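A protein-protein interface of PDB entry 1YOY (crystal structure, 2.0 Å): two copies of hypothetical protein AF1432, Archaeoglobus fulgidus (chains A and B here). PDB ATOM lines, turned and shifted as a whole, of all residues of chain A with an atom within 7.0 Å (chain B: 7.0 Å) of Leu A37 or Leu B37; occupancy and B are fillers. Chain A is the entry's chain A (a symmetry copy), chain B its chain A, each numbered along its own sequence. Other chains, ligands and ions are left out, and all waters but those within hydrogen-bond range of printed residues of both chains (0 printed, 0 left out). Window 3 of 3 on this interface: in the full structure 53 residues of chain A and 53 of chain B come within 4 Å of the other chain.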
ATOM      1  N   LEU A  24      -4.545  -1.966  14.840  1.00  0.00           N
ATOM      2  CA  LEU A  24      -4.620  -3.309  14.310  1.00  0.00           C
ATOM      3  C   LEU A  24      -4.429  -3.279  12.782  1.00  0.00           C
ATOM      4  O   LEU A  24      -4.576  -4.298  12.126  1.00  0.00           O
ATOM      5  CB  LEU A  24      -5.984  -3.929  14.661  1.00  0.00           C
ATOM      6  CG  LEU A  24      -6.245  -3.920  16.165  1.00  0.00           C
ATOM      7  CD1 LEU A  24      -7.673  -4.366  16.434  1.00  0.00           C
ATOM      8  CD2 LEU A  24      -5.187  -4.738  16.927  1.00  0.00           C
ATOM      9  N   PRO A  26      -1.897  -2.748   9.796  1.00  0.00           N
ATOM     10  CA  PRO A  26      -0.485  -2.637   9.438  1.00  0.00           C
ATOM     11  C   PRO A  26      -0.282  -1.566   8.393  1.00  0.00           C
ATOM     12  O   PRO A  26      -1.160  -1.331   7.556  1.00  0.00           O
ATOM     13  CB  PRO A  26      -0.086  -4.041   8.850  1.00  0.00           C
ATOM     14  CG  PRO A  26      -1.373  -4.856   8.791  1.00  0.00           C
ATOM     15  CD  PRO A  26      -2.521  -4.031   9.353  1.00  0.00           C
ATOM     16  N   LEU A  31       5.150  -4.939   4.219  1.00  0.00           N
ATOM     17  CA  LEU A  31       4.846  -6.384   4.232  1.00  0.00           C
ATOM     18  C   LEU A  31       5.511  -7.125   3.109  1.00  0.00           C
ATOM     19  O   LEU A  31       6.096  -8.174   3.354  1.00  0.00           O
ATOM     20  CB  LEU A  31       3.317  -6.679   4.256  1.00  0.00           C
ATOM     21  CG  LEU A  31       2.580  -6.312   5.575  1.00  0.00           C
ATOM     22  CD1 LEU A  31       1.059  -6.135   5.315  1.00  0.00           C
ATOM     23  CD2 LEU A  31       2.821  -7.263   6.725  1.00  0.00           C
ATOM     24  N   GLY A  34       9.051  -8.254   3.515  1.00  0.00           N
ATOM     25  CA  GLY A  34       9.380  -9.361   4.404  1.00  0.00           C
ATOM     26  C   GLY A  34       9.354  -8.986   5.862  1.00  0.00           C
ATOM     27  O   GLY A  34       9.642  -9.818   6.707  1.00  0.00           O
ATOM     28  N   ILE A  35       9.004  -7.739   6.164  1.00  0.00           N
ATOM     29  CA  ILE A  35       8.938  -7.235   7.559  1.00  0.00           C
ATOM     30  C   ILE A  35       7.623  -7.751   8.122  1.00  0.00           C
ATOM     31  O   ILE A  35       6.548  -7.409   7.629  1.00  0.00           O
ATOM     32  CB  ILE A  35       9.078  -5.653   7.628  1.00  0.00           C
ATOM     33  CG1 ILE A  35      10.464  -5.204   7.126  1.00  0.00           C
ATOM     34  CG2 ILE A  35       8.850  -5.121   9.081  1.00  0.00           C
ATOM     35  CD1 ILE A  35      10.477  -3.826   6.490  1.00  0.00           C
ATOM     36  N   ARG A  36       7.693  -8.624   9.126  1.00  0.00           N
ATOM     37  CA  ARG A  36       6.520  -9.410   9.502  1.00  0.00           C
ATOM     38  C   ARG A  36       5.644  -8.720  10.481  1.00  0.00           C
ATOM     39  O   ARG A  36       4.430  -8.930  10.465  1.00  0.00           O
ATOM     40  CB  ARG A  36       6.930 -10.794  10.072  1.00  0.00           C
ATOM     41  CG  ARG A  36       7.557 -11.661   8.982  1.00  0.00           C
ATOM     42  CD  ARG A  36       6.478 -12.264   8.091  1.00  0.00           C
ATOM     43  NE  ARG A  36       6.065 -13.586   8.595  1.00  0.00           N
ATOM     44  CZ  ARG A  36       4.862 -14.146   8.397  1.00  0.00           C
ATOM     45  NH1 ARG A  36       3.905 -13.493   7.744  1.00  0.00           N
ATOM     46  NH2 ARG A  36       4.608 -15.368   8.882  1.00  0.00           N
ATOM     47  N   LEU A  37       6.217  -7.925  11.374  1.00  0.00           N
ATOM     48  CA  LEU A  37       5.316  -7.253  12.289  1.00  0.00           C
ATOM     49  C   LEU A  37       5.600  -5.769  12.183  1.00  0.00           C
ATOM     50  O   LEU A  37       6.294  -5.228  13.025  1.00  0.00           O
ATOM     51  CB  LEU A  37       5.524  -7.768  13.726  1.00  0.00           C
ATOM     52  CG  LEU A  37       5.025  -9.177  14.096  1.00  0.00           C
ATOM     53  CD1 LEU A  37       5.689  -9.579  15.425  1.00  0.00           C
ATOM     54  CD2 LEU A  37       3.522  -9.183  14.268  1.00  0.00           C
ATOM     55  N   PRO A  38       5.190  -5.148  11.060  1.00  0.00           N
ATOM     56  CA  PRO A  38       5.478  -3.736  10.792  1.00  0.00           C
ATOM     57  C   PRO A  38       4.702  -2.784  11.733  1.00  0.00           C
ATOM     58  O   PRO A  38       3.783  -3.213  12.399  1.00  0.00           O
ATOM     59  CB  PRO A  38       5.005  -3.574   9.329  1.00  0.00           C
ATOM     60  CG  PRO A  38       3.869  -4.521   9.273  1.00  0.00           C
ATOM     61  CD  PRO A  38       4.401  -5.730   9.973  1.00  0.00           C
ATOM     62  N   GLU A  39       5.104  -1.503  11.782  1.00  0.00           N
ATOM     63  CA  GLU A  39       4.326  -0.437  12.417  1.00  0.00           C
ATOM     64  C   GLU A  39       2.884  -0.472  11.924  1.00  0.00           C
ATOM     65  O   GLU A  39       2.625  -0.813  10.757  1.00  0.00           O
ATOM     66  CB  GLU A  39       4.934   0.939  12.078  1.00  0.00           C
ATOM     67  CG  GLU A  39       5.159   1.100  10.594  1.00  0.00           C
ATOM     68  CD  GLU A  39       5.061   2.524  10.112  1.00  0.00           C
ATOM     69  OE1 GLU A  39       4.855   3.412  10.947  1.00  0.00           O
ATOM     70  OE2 GLU A  39       5.195   2.774   8.895  1.00  0.00           O
ATOM     71  N   SER A  40       1.953  -0.155  12.826  1.00  0.00           N
ATOM     72  CA  SER A  40       0.566   0.035  12.501  1.00  0.00           C
ATOM     73  C   SER A  40       0.322   1.478  12.017  1.00  0.00           C
ATOM     74  O   SER A  40       1.164   2.369  12.193  1.00  0.00           O
ATOM     75  CB  SER A  40      -0.334  -0.276  13.715  1.00  0.00           C
ATOM     76  OG  SER A  40      -0.143   0.719  14.692  1.00  0.00           O
ATOM     77  N   GLU A  43       0.637   3.851  15.012  1.00  0.00           N
ATOM     78  CA  GLU A  43       2.043   4.152  15.242  1.00  0.00           C
ATOM     79  C   GLU A  43       2.650   5.160  14.275  1.00  0.00           C
ATOM     80  O   GLU A  43       3.338   6.092  14.711  1.00  0.00           O
ATOM     81  CB  GLU A  43       2.867   2.855  15.214  1.00  0.00           C
ATOM     82  CG  GLU A  43       2.620   2.133  16.540  1.00  0.00           C
ATOM     83  CD  GLU A  43       3.120   0.726  16.495  1.00  0.00           C
ATOM     84  OE1 GLU A  43       3.326   0.171  15.391  1.00  0.00           O
ATOM     85  OE2 GLU A  43       3.342   0.199  17.581  1.00  0.00           O
ATOM     86  N   TYR A 137      14.161   0.631   9.439  1.00  0.00           N
ATOM     87  CA  TYR A 137      13.975  -0.719   8.963  1.00  0.00           C
ATOM     88  C   TYR A 137      15.110  -1.173   8.057  1.00  0.00           C
ATOM     89  O   TYR A 137      15.288  -2.363   7.855  1.00  0.00           O
ATOM     90  CB  TYR A 137      12.626  -0.865   8.212  1.00  0.00           C
ATOM     91  CG  TYR A 137      11.367  -0.977   9.042  1.00  0.00           C
ATOM     92  CD1 TYR A 137      11.360  -1.589  10.305  1.00  0.00           C
ATOM     93  CD2 TYR A 137      10.148  -0.558   8.523  1.00  0.00           C
ATOM     94  CE1 TYR A 137      10.187  -1.723  11.062  1.00  0.00           C
ATOM     95  CE2 TYR A 137       8.992  -0.696   9.245  1.00  0.00           C
ATOM     96  CZ  TYR A 137       9.007  -1.310  10.504  1.00  0.00           C
ATOM     97  OH  TYR A 137       7.842  -1.413  11.215  1.00  0.00           O
ATOM     98  N   GLN A 140      17.341  -3.986   9.203  1.00  0.00           N
ATOM     99  CA  GLN A 140      16.871  -5.382   9.035  1.00  0.00           C
ATOM    100  C   GLN A 140      16.784  -5.816   7.581  1.00  0.00           C
ATOM    101  O   GLN A 140      17.037  -6.993   7.235  1.00  0.00           O
ATOM    102  CB  GLN A 140      15.448  -5.514   9.555  1.00  0.00           C
ATOM    103  CG  GLN A 140      15.307  -5.375  11.000  1.00  0.00           C
ATOM    104  CD  GLN A 140      13.939  -4.796  11.308  1.00  0.00           C
ATOM    105  OE1 GLN A 140      13.838  -3.773  11.989  1.00  0.00           O
ATOM    106  NE2 GLN A 140      12.868  -5.442  10.777  1.00  0.00           N
ATOM    107  N   LEU B  24       8.051   0.460  19.680  1.00  0.00           N
ATOM    108  CA  LEU B  24       8.710  -0.788  19.989  1.00  0.00           C
ATOM    109  C   LEU B  24       8.580  -1.088  21.493  1.00  0.00           C
ATOM    110  O   LEU B  24       9.171  -2.040  21.982  1.00  0.00           O
ATOM    111  CB  LEU B  24      10.195  -0.701  19.592  1.00  0.00           C
ATOM    112  CG  LEU B  24      10.372  -0.340  18.120  1.00  0.00           C
ATOM    113  CD1 LEU B  24      11.843  -0.086  17.834  1.00  0.00           C
ATOM    114  CD2 LEU B  24       9.737  -1.396  17.198  1.00  0.00           C
ATOM    115  N   PRO B  26       6.174  -2.177  24.432  1.00  0.00           N
ATOM    116  CA  PRO B  26       4.864  -2.738  24.752  1.00  0.00           C
ATOM    117  C   PRO B  26       4.262  -2.039  25.947  1.00  0.00           C
ATOM    118  O   PRO B  26       4.985  -1.591  26.843  1.00  0.00           O
ATOM    119  CB  PRO B  26       5.122  -4.252  25.091  1.00  0.00           C
ATOM    120  CG  PRO B  26       6.635  -4.439  25.064  1.00  0.00           C
ATOM    121  CD  PRO B  26       7.301  -3.125  24.685  1.00  0.00           C
ATOM    122  N   LEU B  31       0.941  -8.030  29.324  1.00  0.00           N
ATOM    123  CA  LEU B  31       1.831  -9.184  29.088  1.00  0.00           C
ATOM    124  C   LEU B  31       1.586 -10.308  30.051  1.00  0.00           C
ATOM    125  O   LEU B  31       1.496 -11.453  29.620  1.00  0.00           O
ATOM    126  CB  LEU B  31       3.338  -8.792  29.073  1.00  0.00           C
ATOM    127  CG  LEU B  31       3.800  -7.938  27.857  1.00  0.00           C
ATOM    128  CD1 LEU B  31       5.109  -7.174  28.198  1.00  0.00           C
ATOM    129  CD2 LEU B  31       3.945  -8.702  26.561  1.00  0.00           C
ATOM    130  N   GLY B  34      -1.147 -12.758  29.340  1.00  0.00           N
ATOM    131  CA  GLY B  34      -1.005 -13.739  28.274  1.00  0.00           C
ATOM    132  C   GLY B  34      -1.194 -13.160  26.896  1.00  0.00           C
ATOM    133  O   GLY B  34      -1.131 -13.886  25.918  1.00  0.00           O
ATOM    134  N   ILE B  35      -1.420 -11.852  26.813  1.00  0.00           N
ATOM    135  CA  ILE B  35      -1.627 -11.149  25.520  1.00  0.00           C
ATOM    136  C   ILE B  35      -0.239 -10.958  24.930  1.00  0.00           C
ATOM    137  O   ILE B  35       0.606 -10.274  25.511  1.00  0.00           O
ATOM    138  CB  ILE B  35      -2.430  -9.790  25.702  1.00  0.00           C
ATOM    139  CG1 ILE B  35      -3.855 -10.063  26.220  1.00  0.00           C
ATOM    140  CG2 ILE B  35      -2.503  -8.985  24.364  1.00  0.00           C
ATOM    141  CD1 ILE B  35      -4.431  -8.943  27.069  1.00  0.00           C
ATOM    142  N   ARG B  36       0.034 -11.602  23.796  1.00  0.00           N
ATOM    143  CA  ARG B  36       1.416 -11.742  23.342  1.00  0.00           C
ATOM    144  C   ARG B  36       1.878 -10.596  22.519  1.00  0.00           C
ATOM    145  O   ARG B  36       3.066 -10.269  22.545  1.00  0.00           O
ATOM    146  CB  ARG B  36       1.614 -13.056  22.541  1.00  0.00           C
ATOM    147  CG  ARG B  36       1.457 -14.272  23.454  1.00  0.00           C
ATOM    148  CD  ARG B  36       2.721 -14.492  24.275  1.00  0.00           C
ATOM    149  NE  ARG B  36       3.639 -15.411  23.578  1.00  0.00           N
ATOM    150  CZ  ARG B  36       4.972 -15.430  23.727  1.00  0.00           C
ATOM    151  NH1 ARG B  36       5.583 -14.545  24.512  1.00  0.00           N
ATOM    152  NH2 ARG B  36       5.706 -16.330  23.062  1.00  0.00           N
ATOM    153  N   LEU B  37       0.989  -9.989  21.746  1.00  0.00           N
ATOM    154  CA  LEU B  37       1.484  -8.859  20.984  1.00  0.00           C
ATOM    155  C   LEU B  37       0.598  -7.676  21.318  1.00  0.00           C
ATOM    156  O   LEU B  37      -0.290  -7.355  20.549  1.00  0.00           O
ATOM    157  CB  LEU B  37       1.463  -9.174  19.477  1.00  0.00           C
ATOM    158  CG  LEU B  37       2.500 -10.156  18.903  1.00  0.00           C
ATOM    159  CD1 LEU B  37       2.023 -10.583  17.504  1.00  0.00           C
ATOM    160  CD2 LEU B  37       3.856  -9.493  18.787  1.00  0.00           C
ATOM    161  N   PRO B  38       0.745  -7.130  22.540  1.00  0.00           N
ATOM    162  CA  PRO B  38      -0.107  -6.039  23.022  1.00  0.00           C
ATOM    163  C   PRO B  38       0.154  -4.709  22.276  1.00  0.00           C
ATOM    164  O   PRO B  38       1.143  -4.592  21.583  1.00  0.00           O
ATOM    165  CB  PRO B  38       0.304  -5.930  24.509  1.00  0.00           C
ATOM    166  CG  PRO B  38       1.736  -6.297  24.453  1.00  0.00           C
ATOM    167  CD  PRO B  38       1.746  -7.487  23.548  1.00  0.00           C
ATOM    168  N   GLU B  39      -0.757  -3.732  22.420  1.00  0.00           N
ATOM    169  CA  GLU B  39      -0.531  -2.349  21.994  1.00  0.00           C
ATOM    170  C   GLU B  39       0.805  -1.845  22.526  1.00  0.00           C
ATOM    171  O   GLU B  39       1.227  -2.227  23.632  1.00  0.00           O
ATOM    172  CB  GLU B  39      -1.655  -1.438  22.528  1.00  0.00           C
ATOM    173  CG  GLU B  39      -1.873  -1.629  24.009  1.00  0.00           C
ATOM    174  CD  GLU B  39      -2.374  -0.398  24.717  1.00  0.00           C
ATOM    175  OE1 GLU B  39      -2.596   0.614  24.044  1.00  0.00           O
ATOM    176  OE2 GLU B  39      -2.557  -0.429  25.953  1.00  0.00           O
ATOM    177  N   SER B  40       1.478  -1.021  21.721  1.00  0.00           N
ATOM    178  CA  SER B  40       2.663  -0.313  22.124  1.00  0.00           C
ATOM    179  C   SER B  40       2.286   0.997  22.842  1.00  0.00           C
ATOM    180  O   SER B  40       1.140   1.460  22.782  1.00  0.00           O
ATOM    181  CB  SER B  40       3.565  -0.011  20.909  1.00  0.00           C
ATOM    182  OG  SER B  40       2.934   0.951  20.100  1.00  0.00           O
ATOM    183  N   GLU B  43       0.882   3.458  20.260  1.00  0.00           N
ATOM    184  CA  GLU B  43      -0.526   3.164  20.031  1.00  0.00           C
ATOM    185  C   GLU B  43      -1.470   3.647  21.125  1.00  0.00           C
ATOM    186  O   GLU B  43      -2.504   4.254  20.820  1.00  0.00           O
ATOM    187  CB  GLU B  43      -0.717   1.654  19.819  1.00  0.00           C
ATOM    188  CG  GLU B  43      -0.234   1.331  18.404  1.00  0.00           C
ATOM    189  CD  GLU B  43      -0.085  -0.143  18.203  1.00  0.00           C
ATOM    190  OE1 GLU B  43       0.005  -0.902  19.195  1.00  0.00           O
ATOM    191  OE2 GLU B  43      -0.101  -0.532  17.039  1.00  0.00           O
ATOM    192  N   TYR B 137      -9.768  -6.070  24.745  1.00  0.00           N
ATOM    193  CA  TYR B 137      -9.007  -7.269  25.003  1.00  0.00           C
ATOM    194  C   TYR B 137      -9.806  -8.304  25.782  1.00  0.00           C
ATOM    195  O   TYR B 137      -9.453  -9.471  25.784  1.00  0.00           O
ATOM    196  CB  TYR B 137      -7.698  -6.945  25.770  1.00  0.00           C
ATOM    197  CG  TYR B 137      -6.542  -6.375  24.979  1.00  0.00           C
ATOM    198  CD1 TYR B 137      -6.321  -6.713  23.634  1.00  0.00           C
ATOM    199  CD2 TYR B 137      -5.601  -5.566  25.603  1.00  0.00           C
ATOM    200  CE1 TYR B 137      -5.231  -6.210  22.910  1.00  0.00           C
ATOM    201  CE2 TYR B 137      -4.523  -5.080  24.911  1.00  0.00           C
ATOM    202  CZ  TYR B 137      -4.320  -5.429  23.569  1.00  0.00           C
ATOM    203  OH  TYR B 137      -3.249  -4.911  22.894  1.00  0.00           O
ATOM    204  N   GLN B 140     -10.666 -11.574  24.118  1.00  0.00           N
ATOM    205  CA  GLN B 140      -9.640 -12.642  24.075  1.00  0.00           C
ATOM    206  C   GLN B 140      -9.323 -13.226  25.442  1.00  0.00           C
ATOM    207  O   GLN B 140      -9.038 -14.437  25.585  1.00  0.00           O
ATOM    208  CB  GLN B 140      -8.316 -12.070  23.593  1.00  0.00           C
ATOM    209  CG  GLN B 140      -8.301 -11.653  22.195  1.00  0.00           C
ATOM    210  CD  GLN B 140      -7.322 -10.505  22.035  1.00  0.00           C
ATOM    211  OE1 GLN B 140      -7.693  -9.441  21.532  1.00  0.00           O
ATOM    212  NE2 GLN B 140      -6.059 -10.709  22.494  1.00  0.00           N
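The side-chain hydroxyl (OG) of Ser B40 is in hydrogen-bond range of the side-chain carboxylate (OE2) of Glu A43, at 2.7 Å.
OE2 of Glu B43 is in hydrogen-bond range of OG of Ser A40.
The side-chain carboxylate (OE1) of Glu B43 is in hydrogen-bond range of the backbone NH (N) of Ser B40, 2.9 Å away.
N of Ser A40 lies within hydrogen-bond range of OE1 of Glu A43, 2.9 Å away.
Among the printed residues, merely in contact across the chains: Leu A37 with Leu B37 (3.8 Å) and Glu A43 with Glu B43 (3.5 Å).
Leu A37 touches one residue of chain B.
Of the printed residues of chain A, Leu B37 touches Leu A37.
Of the printed residues of chain A, Ser B40 touches Glu A43 (2.7 Å).
Of the printed residues of chain B, Ser A40 touches Glu B43.
Of the printed residues of chain A, Glu B43 touches Ser A40 (2.7 Å) and Glu A43 (3.5 Å).
Of the printed residues of chain B, Glu A43 touches Ser B40 and Glu B43.
Gln B140 touches none of the printed residues of chain A.
The nearest residue of chain B that does not touch Leu A37 is Leu B24 (6.6 Å).
The nearest printed residue of chain B that does not touch Glu A43 is Leu B24 (5.2 Å).
Of the 13 printed residues of chain A, 3 touch a printed residue of chain B.
Printed residues of chain A that touch a printed residue of chain B: Leu A37, Ser A40 and Glu A43.
Hydrophobic or aromatic side chains of chain A that line the printed part of chain B: Leu A37.
Hydrophobic or aromatic side chains of chain B that line the printed part of chain A: Leu B37.
Among the printed residues, 4 pairs touch across the chains.
Among the printed residues, no Asp or Glu carboxylate lies within 4 Å of a Lys or Arg side-chain nitrogen of the other chain.
Leu B37 touches its own counterpart, Leu A37.
Ser A40 touches Glu B43, and with the chains exchanged Glu A43 touches Ser B40.
Glu B43 touches its own counterpart, Glu A43.
Of the 4 pairs that touch across the chains among the printed residues, 4 have their exchanged pair printed and touching as well.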
